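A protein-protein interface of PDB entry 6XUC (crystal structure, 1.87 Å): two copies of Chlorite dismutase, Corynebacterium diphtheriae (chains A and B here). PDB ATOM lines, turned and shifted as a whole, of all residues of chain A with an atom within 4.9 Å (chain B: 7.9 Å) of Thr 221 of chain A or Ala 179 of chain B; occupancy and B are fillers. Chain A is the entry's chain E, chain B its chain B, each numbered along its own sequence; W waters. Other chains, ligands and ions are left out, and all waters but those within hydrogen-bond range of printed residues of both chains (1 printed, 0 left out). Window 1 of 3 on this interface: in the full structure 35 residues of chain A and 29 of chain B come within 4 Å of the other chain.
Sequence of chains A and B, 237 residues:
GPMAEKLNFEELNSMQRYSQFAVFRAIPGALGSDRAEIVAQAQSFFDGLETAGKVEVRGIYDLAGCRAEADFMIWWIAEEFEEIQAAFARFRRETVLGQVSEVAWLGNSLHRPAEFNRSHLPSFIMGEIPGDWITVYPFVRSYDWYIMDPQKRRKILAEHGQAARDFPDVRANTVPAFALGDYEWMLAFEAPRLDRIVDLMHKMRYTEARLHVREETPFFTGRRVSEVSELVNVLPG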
ATOM      1  N   ASP A  62      27.420  12.444  -1.804  1.00  0.00           N
ATOM      2  CA  ASP A  62      26.769  11.139  -1.810  1.00  0.00           C
ATOM      3  C   ASP A  62      25.911  11.021  -0.556  1.00  0.00           C
ATOM      4  O   ASP A  62      26.437  10.944   0.561  1.00  0.00           O
ATOM      5  CB  ASP A  62      27.813  10.024  -1.851  1.00  0.00           C
ATOM      6  CG  ASP A  62      27.198   8.634  -1.849  1.00  0.00           C
ATOM      7  OD1 ASP A  62      25.952   8.522  -1.842  1.00  0.00           O
ATOM      8  OD2 ASP A  62      27.970   7.640  -1.840  1.00  0.00           O
ATOM      9  N   LEU A  63      24.592  10.967  -0.728  1.00  0.00           N
ATOM     10  CA  LEU A  63      23.700  10.748   0.403  1.00  0.00           C
ATOM     11  C   LEU A  63      23.239   9.310   0.554  1.00  0.00           C
ATOM     12  O   LEU A  63      22.303   9.058   1.320  1.00  0.00           O
ATOM     13  CB  LEU A  63      22.453  11.639   0.299  1.00  0.00           C
ATOM     14  CG  LEU A  63      22.712  13.139   0.103  1.00  0.00           C
ATOM     15  CD1 LEU A  63      21.389  13.868  -0.022  1.00  0.00           C
ATOM     16  CD2 LEU A  63      23.579  13.756   1.172  1.00  0.00           C
ATOM     17  N   CYS A  66      21.252   7.640   3.575  1.00  0.00           N
ATOM     18  CA  CYS A  66      20.819   8.562   4.618  1.00  0.00           C
ATOM     19  C   CYS A  66      19.313   8.451   4.828  1.00  0.00           C
ATOM     20  O   CYS A  66      18.856   8.197   5.951  1.00  0.00           O
ATOM     21  CB  CYS A  66      21.221  10.001   4.309  1.00  0.00           C
ATOM     22  SG  CYS A  66      20.243  11.186   5.325  1.00  0.00           S
ATOM     23  N   ILE A 134      29.005  16.029   5.831  1.00  0.00           N
ATOM     24  CA  ILE A 134      28.093  17.151   5.992  1.00  0.00           C
ATOM     25  C   ILE A 134      26.725  16.669   6.440  1.00  0.00           C
ATOM     26  O   ILE A 134      26.235  15.628   5.984  1.00  0.00           O
ATOM     27  CB  ILE A 134      27.953  17.959   4.690  1.00  0.00           C
ATOM     28  CG1 ILE A 134      27.505  19.385   4.984  1.00  0.00           C
ATOM     29  CG2 ILE A 134      26.952  17.287   3.727  1.00  0.00           C
ATOM     30  CD1 ILE A 134      27.587  20.271   3.776  1.00  0.00           C
ATOM     31  N   THR A 135      26.118  17.408   7.364  1.00  0.00           N
ATOM     32  CA  THR A 135      24.686  17.330   7.583  1.00  0.00           C
ATOM     33  C   THR A 135      24.082  18.703   7.318  1.00  0.00           C
ATOM     34  O   THR A 135      24.624  19.724   7.762  1.00  0.00           O
ATOM     35  CB  THR A 135      24.295  16.891   8.989  1.00  0.00           C
ATOM     36  OG1 THR A 135      22.927  16.453   8.962  1.00  0.00           O
ATOM     37  CG2 THR A 135      24.408  18.027   9.960  1.00  0.00           C
ATOM     38  N   LEU A 194      31.994  11.709  10.341  1.00  0.00           N
ATOM     39  CA  LEU A 194      30.565  11.769  10.637  1.00  0.00           C
ATOM     40  C   LEU A 194      30.293  11.737  12.137  1.00  0.00           C
ATOM     41  O   LEU A 194      29.372  12.397  12.612  1.00  0.00           O
ATOM     42  CB  LEU A 194      29.860  10.613   9.916  1.00  0.00           C
ATOM     43  CG  LEU A 194      28.331  10.541  10.059  1.00  0.00           C
ATOM     44  CD1 LEU A 194      27.746  11.894   9.808  1.00  0.00           C
ATOM     45  CD2 LEU A 194      27.761   9.527   9.103  1.00  0.00           C
ATOM     46  N   ILE A 197      29.851  14.999  13.984  1.00  0.00           N
ATOM     47  CA  ILE A 197      28.562  15.656  13.760  1.00  0.00           C
ATOM     48  C   ILE A 197      27.480  15.067  14.647  1.00  0.00           C
ATOM     49  O   ILE A 197      26.664  15.798  15.231  1.00  0.00           O
ATOM     50  CB  ILE A 197      28.155  15.562  12.279  1.00  0.00           C
ATOM     51  CG1 ILE A 197      29.230  16.175  11.360  1.00  0.00           C
ATOM     52  CG2 ILE A 197      26.841  16.272  12.074  1.00  0.00           C
ATOM     53  CD1 ILE A 197      28.841  16.128   9.881  1.00  0.00           C
ATOM     54  N   VAL A 198      27.398  13.731  14.705  1.00  0.00           N
ATOM     55  CA  VAL A 198      26.434  13.102  15.599  1.00  0.00           C
ATOM     56  C   VAL A 198      26.658  13.596  17.020  1.00  0.00           C
ATOM     57  O   VAL A 198      25.726  14.025  17.701  1.00  0.00           O
ATOM     58  CB  VAL A 198      26.529  11.569  15.499  1.00  0.00           C
ATOM     59  CG1 VAL A 198      25.555  10.878  16.434  1.00  0.00           C
ATOM     60  CG2 VAL A 198      26.276  11.152  14.045  1.00  0.00           C
ATOM     61  N   MET A 201      25.566  17.332  17.637  1.00  0.00           N
ATOM     62  CA  MET A 201      24.125  17.543  17.740  1.00  0.00           C
ATOM     63  C   MET A 201      23.620  17.019  19.091  1.00  0.00           C
ATOM     64  O   MET A 201      22.797  17.657  19.745  1.00  0.00           O
ATOM     65  CB  MET A 201      23.360  16.898  16.578  1.00  0.00           C
ATOM     66  CG  MET A 201      23.730  17.345  15.183  1.00  0.00           C
ATOM     67  SD  MET A 201      23.471  19.051  14.923  1.00  0.00           S
ATOM     68  CE  MET A 201      21.896  19.324  15.974  1.00  0.00           C
ATOM     69  N   PHE A 219      16.556  16.236   7.377  1.00  0.00           N
ATOM     70  CA  PHE A 219      18.008  16.152   7.420  1.00  0.00           C
ATOM     71  C   PHE A 219      18.573  15.458   6.178  1.00  0.00           C
ATOM     72  O   PHE A 219      18.035  14.456   5.712  1.00  0.00           O
ATOM     73  CB  PHE A 219      18.485  15.336   8.628  1.00  0.00           C
ATOM     74  CG  PHE A 219      18.596  16.091   9.921  1.00  0.00           C
ATOM     75  CD1 PHE A 219      17.464  16.415  10.664  1.00  0.00           C
ATOM     76  CD2 PHE A 219      19.849  16.413  10.441  1.00  0.00           C
ATOM     77  CE1 PHE A 219      17.597  17.106  11.868  1.00  0.00           C
ATOM     78  CE2 PHE A 219      19.977  17.068  11.666  1.00  0.00           C
ATOM     79  CZ  PHE A 219      18.854  17.413  12.366  1.00  0.00           C
ATOM     80  N   PHE A 220      19.715  15.954   5.701  1.00  0.00           N
ATOM     81  CA  PHE A 220      20.468  15.339   4.608  1.00  0.00           C
ATOM     82  C   PHE A 220      21.925  15.260   5.041  1.00  0.00           C
ATOM     83  O   PHE A 220      22.563  16.285   5.329  1.00  0.00           O
ATOM     84  CB  PHE A 220      20.311  16.120   3.295  1.00  0.00           C
ATOM     85  CG  PHE A 220      18.867  16.354   2.915  1.00  0.00           C
ATOM     86  CD1 PHE A 220      18.178  15.438   2.164  1.00  0.00           C
ATOM     87  CD2 PHE A 220      18.210  17.503   3.336  1.00  0.00           C
ATOM     88  CE1 PHE A 220      16.865  15.644   1.840  1.00  0.00           C
ATOM     89  CE2 PHE A 220      16.918  17.725   3.024  1.00  0.00           C
ATOM     90  CZ  PHE A 220      16.223  16.809   2.261  1.00  0.00           C
ATOM     91  N   THR A 221      22.426  14.036   5.125  1.00  0.00           N
ATOM     92  CA  THR A 221      23.742  13.742   5.658  1.00  0.00           C
ATOM     93  C   THR A 221      24.454  12.903   4.640  1.00  0.00           C
ATOM     94  O   THR A 221      23.869  11.956   4.109  1.00  0.00           O
ATOM     95  CB  THR A 221      23.599  13.014   6.984  1.00  0.00           C
ATOM     96  OG1 THR A 221      22.873  13.875   7.865  1.00  0.00           O
ATOM     97  CG2 THR A 221      24.920  12.675   7.549  1.00  0.00           C
ATOM     98  N   GLY A 222      25.704  13.254   4.352  1.00  0.00           N
ATOM     99  CA  GLY A 222      26.427  12.474   3.381  1.00  0.00           C
ATOM    100  C   GLY A 222      27.860  12.919   3.230  1.00  0.00           C
ATOM    101  O   GLY A 222      28.351  13.824   3.921  1.00  0.00           O
ATOM    102  N   ARG A 223      28.507  12.276   2.267  1.00  0.00           N
ATOM    103  CA  ARG A 223      29.938  12.324   2.089  1.00  0.00           C
ATOM    104  C   ARG A 223      30.293  13.120   0.842  1.00  0.00           C
ATOM    105  O   ARG A 223      29.737  12.887  -0.237  1.00  0.00           O
ATOM    106  CB  ARG A 223      30.489  10.900   1.987  1.00  0.00           C
ATOM    107  CG  ARG A 223      32.001  10.850   1.754  1.00  0.00           C
ATOM    108  CD  ARG A 223      32.482   9.414   1.480  1.00  0.00           C
ATOM    109  NE  ARG A 223      32.240   8.988   0.101  1.00  0.00           N
ATOM    110  CZ  ARG A 223      31.249   8.183  -0.283  1.00  0.00           C
ATOM    111  NH1 ARG A 223      30.386   7.694   0.600  1.00  0.00           N
ATOM    112  NH2 ARG A 223      31.120   7.863  -1.563  1.00  0.00           N
ATOM    113  N   PHE B  81      30.474   4.356   8.634  1.00  0.00           N
ATOM    114  CA  PHE B  81      29.248   4.581   7.899  1.00  0.00           C
ATOM    115  C   PHE B  81      29.427   4.327   6.409  1.00  0.00           C
ATOM    116  O   PHE B  81      28.545   3.742   5.768  1.00  0.00           O
ATOM    117  CB  PHE B  81      28.687   5.984   8.114  1.00  0.00           C
ATOM    118  CG  PHE B  81      27.254   6.079   7.663  1.00  0.00           C
ATOM    119  CD1 PHE B  81      26.274   5.283   8.266  1.00  0.00           C
ATOM    120  CD2 PHE B  81      26.889   6.874   6.604  1.00  0.00           C
ATOM    121  CE1 PHE B  81      25.007   5.286   7.828  1.00  0.00           C
ATOM    122  CE2 PHE B  81      25.588   6.908   6.180  1.00  0.00           C
ATOM    123  CZ  PHE B  81      24.639   6.117   6.796  1.00  0.00           C
ATOM    124  N   GLN B  85      27.119   2.593   3.547  1.00  0.00           N
ATOM    125  CA  GLN B  85      26.704   3.293   2.332  1.00  0.00           C
ATOM    126  C   GLN B  85      27.029   2.466   1.109  1.00  0.00           C
ATOM    127  O   GLN B  85      26.182   2.284   0.218  1.00  0.00           O
ATOM    128  CB  GLN B  85      27.405   4.647   2.190  1.00  0.00           C
ATOM    129  CG  GLN B  85      27.026   5.720   3.140  1.00  0.00           C
ATOM    130  CD  GLN B  85      27.647   7.032   2.724  1.00  0.00           C
ATOM    131  OE1 GLN B  85      28.840   7.214   2.884  1.00  0.00           O
ATOM    132  NE2 GLN B  85      26.845   7.936   2.147  1.00  0.00           N
ATOM    133  N   ASN B 108      19.148   5.068  10.763  1.00  0.00           N
ATOM    134  CA  ASN B 108      20.587   5.048  10.994  1.00  0.00           C
ATOM    135  C   ASN B 108      20.886   5.447  12.425  1.00  0.00           C
ATOM    136  O   ASN B 108      20.158   6.257  13.028  1.00  0.00           O
ATOM    137  CB  ASN B 108      21.294   6.011  10.038  1.00  0.00           C
ATOM    138  CG  ASN B 108      21.061   5.639   8.577  1.00  0.00           C
ATOM    139  OD1 ASN B 108      21.353   4.513   8.163  1.00  0.00           O
ATOM    140  ND2 ASN B 108      20.517   6.560   7.804  1.00  0.00           N
ATOM    141  N   PRO B 176      21.877   6.319  19.654  1.00  0.00           N
ATOM    142  CA  PRO B 176      21.741   7.680  19.126  1.00  0.00           C
ATOM    143  C   PRO B 176      21.574   7.697  17.620  1.00  0.00           C
ATOM    144  O   PRO B 176      22.286   7.000  16.887  1.00  0.00           O
ATOM    145  CB  PRO B 176      23.058   8.361  19.537  1.00  0.00           C
ATOM    146  CG  PRO B 176      23.443   7.682  20.751  1.00  0.00           C
ATOM    147  CD  PRO B 176      23.001   6.239  20.620  1.00  0.00           C
ATOM    148  N   ALA B 177      20.735   8.620  17.156  1.00  0.00           N
ATOM    149  CA  ALA B 177      20.518   8.797  15.728  1.00  0.00           C
ATOM    150  C   ALA B 177      20.593  10.257  15.270  1.00  0.00           C
ATOM    151  O   ALA B 177      20.298  10.547  14.096  1.00  0.00           O
ATOM    152  CB  ALA B 177      19.179   8.169  15.349  1.00  0.00           C
ATOM    153  N   PHE B 178      21.040  11.153  16.136  1.00  0.00           N
ATOM    154  CA  PHE B 178      21.186  12.577  15.806  1.00  0.00           C
ATOM    155  C   PHE B 178      21.937  12.782  14.494  1.00  0.00           C
ATOM    156  O   PHE B 178      23.009  12.228  14.289  1.00  0.00           O
ATOM    157  CB  PHE B 178      21.929  13.307  16.928  1.00  0.00           C
ATOM    158  CG  PHE B 178      21.271  13.149  18.295  1.00  0.00           C
ATOM    159  CD1 PHE B 178      20.205  13.932  18.670  1.00  0.00           C
ATOM    160  CD2 PHE B 178      21.725  12.180  19.163  1.00  0.00           C
ATOM    161  CE1 PHE B 178      19.583  13.742  19.930  1.00  0.00           C
ATOM    162  CE2 PHE B 178      21.134  11.980  20.393  1.00  0.00           C
ATOM    163  CZ  PHE B 178      20.085  12.751  20.777  1.00  0.00           C
ATOM    164  N   ALA B 179      21.359  13.569  13.592  1.00  0.00           N
ATOM    165  CA  ALA B 179      21.968  13.919  12.312  1.00  0.00           C
ATOM    166  C   ALA B 179      22.189  12.753  11.347  1.00  0.00           C
ATOM    167  O   ALA B 179      22.762  12.955  10.277  1.00  0.00           O
ATOM    168  CB  ALA B 179      23.316  14.634  12.513  1.00  0.00           C
ATOM    169  N   LEU B 180      21.702  11.547  11.637  1.00  0.00           N
ATOM    170  CA  LEU B 180      21.721  10.499  10.632  1.00  0.00           C
ATOM    171  C   LEU B 180      20.357  10.326   9.953  1.00  0.00           C
ATOM    172  O   LEU B 180      20.055   9.257   9.408  1.00  0.00           O
ATOM    173  CB  LEU B 180      22.188   9.183  11.249  1.00  0.00           C
ATOM    174  CG  LEU B 180      23.438   9.379  12.076  1.00  0.00           C
ATOM    175  CD1 LEU B 180      23.772   8.126  12.875  1.00  0.00           C
ATOM    176  CD2 LEU B 180      24.588   9.712  11.122  1.00  0.00           C
ATOM    177  N   GLY B 181      19.561  11.374   9.939  1.00  0.00           N
ATOM    178  CA  GLY B 181      18.152  11.266   9.638  1.00  0.00           C
ATOM    179  C   GLY B 181      17.375  12.267  10.456  1.00  0.00           C
ATOM    180  O   GLY B 181      17.943  13.163  11.074  1.00  0.00           O
ATOM    181  N   ASP B 182      16.049  12.071  10.511  1.00  0.00           N
ATOM    182  CA  ASP B 182      15.151  13.033  11.136  1.00  0.00           C
ATOM    183  C   ASP B 182      14.929  12.794  12.623  1.00  0.00           C
ATOM    184  O   ASP B 182      14.046  13.433  13.212  1.00  0.00           O
ATOM    185  CB  ASP B 182      13.786  13.029  10.433  1.00  0.00           C
ATOM    186  CG  ASP B 182      13.855  13.529   9.003  1.00  0.00           C
ATOM    187  OD1 ASP B 182      14.875  14.151   8.577  1.00  0.00           O
ATOM    188  OD2 ASP B 182      12.883  13.270   8.290  1.00  0.00           O
ATOM    189  N   TYR B 183      15.724  11.937  13.261  1.00  0.00           N
ATOM    190  CA  TYR B 183      15.359  11.414  14.568  1.00  0.00           C
ATOM    191  C   TYR B 183      16.497  11.590  15.549  1.00  0.00           C
ATOM    192  O   TYR B 183      17.610  11.949  15.178  1.00  0.00           O
ATOM    193  CB  TYR B 183      14.965   9.938  14.470  1.00  0.00           C
ATOM    194  CG  TYR B 183      13.995   9.714  13.366  1.00  0.00           C
ATOM    195  CD1 TYR B 183      12.686  10.175  13.474  1.00  0.00           C
ATOM    196  CD2 TYR B 183      14.374   9.046  12.211  1.00  0.00           C
ATOM    197  CE1 TYR B 183      11.767   9.976  12.434  1.00  0.00           C
ATOM    198  CE2 TYR B 183      13.475   8.851  11.173  1.00  0.00           C
ATOM    199  CZ  TYR B 183      12.176   9.306  11.293  1.00  0.00           C
ATOM    200  OH  TYR B 183      11.294   9.094  10.264  1.00  0.00           O
ATOM    201  N   GLU B 184      16.203  11.295  16.820  1.00  0.00           N
ATOM    202  CA  GLU B 184      17.198  11.368  17.879  1.00  0.00           C
ATOM    203  C   GLU B 184      17.728  10.016  18.321  1.00  0.00           C
ATOM    204  O   GLU B 184      18.898   9.927  18.710  1.00  0.00           O
ATOM    205  CB  GLU B 184      16.627  12.097  19.095  1.00  0.00           C
ATOM    206  CG  GLU B 184      16.303  13.564  18.797  1.00  0.00           C
ATOM    207  CD  GLU B 184      15.663  14.299  19.971  1.00  0.00           C
ATOM    208  OE1 GLU B 184      15.300  13.641  20.978  1.00  0.00           O
ATOM    209  OE2 GLU B 184      15.519  15.549  19.852  1.00  0.00           O
HETATM  210  O   HOH W   1      27.521   4.847  -1.620  1.00  0.00           O
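The backbone carbonyl oxygen of Ala 179 of chain B is in hydrogen-bond range of the side-chain hydroxyl of Thr 221 of chain A, 2.6 Å away.
The side-chain amide oxygen of Gln 85 of chain B is in hydrogen-bond range of the guanidinium group of Arg 223 of chain A (2.8 Å).
N of Phe 219 of chain A sits at hydrogen-bond distance from OD1 of Asp 182 of chain B (2.9 Å).
The side-chain amide nitrogen of Gln 85 of chain B sits at hydrogen-bond distance from the backbone carbonyl oxygen of Asp 62 of chain A (3.4 Å).
The side-chain amide nitrogen (ND2) of Asn 108 of chain B is in hydrogen-bond range of the backbone carbonyl oxygen (O) of Cys 66 of chain A (3.0 Å).
The side-chain hydroxyl (OG1) of Thr 135 of chain A lies within hydrogen-bond range of the side-chain hydroxyl (OG1) of Thr 221 of chain A, 2.8 Å away.
The side-chain sulfur (SG) of Cys 66 of chain A is in hydrogen-bond range of the backbone NH (N) of Thr 221 of chain A (3.6 Å).
The guanidinium group (NH2) of Arg 223 of chain A is in salt-bridge range of the side-chain carboxylate (OD2) of Asp 62 of chain A, at 3.2 Å.
O of Leu 180 of chain B is in hydrogen-bond range of ND2 of Asn 108 of chain B, 3.2 Å away.
Among the printed residues, pairs that only touch across the chains: Phe 219 of chain A with Gly 181 of chain B (3.2 Å), Val 198 of chain A with Phe 178 of chain B (3.4 Å), Val 198 of chain A with Leu 180 of chain B (3.7 Å), Thr 135 of chain A with Ala 179 of chain B (3.7 Å), Leu 194 of chain A with Phe 81 of chain B (3.7 Å), Leu 194 of chain A with Leu 180 of chain B (3.8 Å), Phe 219 of chain A with Ala 179 of chain B (3.8 Å), Cys 66 of chain A with Leu 180 of chain B (3.8 Å), Met 201 of chain A with Ala 179 of chain B (3.8 Å), Met 201 of chain A with Phe 178 of chain B (3.9 Å) and Ile 197 of chain A with Ala 179 of chain B (3.9 Å).
Printed residues of chain A within 4 Å of Ala 179 of chain B: Thr 135 (3.7 Å), Ile 197 (3.9 Å), Met 201 (3.8 Å), Phe 219 (3.8 Å) and Thr 221 (2.6 Å).
Printed residues of chain B within 4 Å of Arg 223 of chain A: Gln 85 (2.8 Å).
Of the printed residues of chain B, Leu 194 of chain A touches Phe 81 (3.7 Å) and Leu 180 (3.8 Å).
Of the printed residues of chain B, Met 201 of chain A touches Phe 178 (3.9 Å) and Ala 179 (3.8 Å).
Tyr 183 of chain B touches none of the printed residues of chain A.
The nearest residue of chain B that does not touch Thr 221 of chain A is Leu 180 of chain B (4.5 Å).
The nearest printed residue of chain A that does not touch Ala 179 of chain B is Val 198 of chain A (4.6 Å).
Of the 12 printed residues of chain B, 8 touch a printed residue of chain A.
Printed residues of chain A that touch a printed residue of chain B: Asp 62, Cys 66, Thr 135, Leu 194, Ile 197, Val 198, Met 201, Phe 219, Thr 221 and Arg 223.
Hydrophobic or aromatic side chains of chain A within 4 Å of the printed part of chain B: Leu 194, Ile 197, Val 198, Met 201 and Phe 219.
Among the printed residues, 16 pairs touch across the chains.
Among the printed residues, no Asp or Glu carboxylate lies within 4 Å of a Lys or Arg side-chain nitrogen of the other chain.
No position is printed for both chains.
Of the 16 pairs that touch across the chains among the printed residues, none has its exchanged pair printed and touching as well.
Water W1 lies within hydrogen-bond range of the side-chain carboxylate (OD2) of Asp 62 of chain A (2.8 Å) and the backbone carbonyl oxygen (O) of Gln 85 of chain B (3.4 Å).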
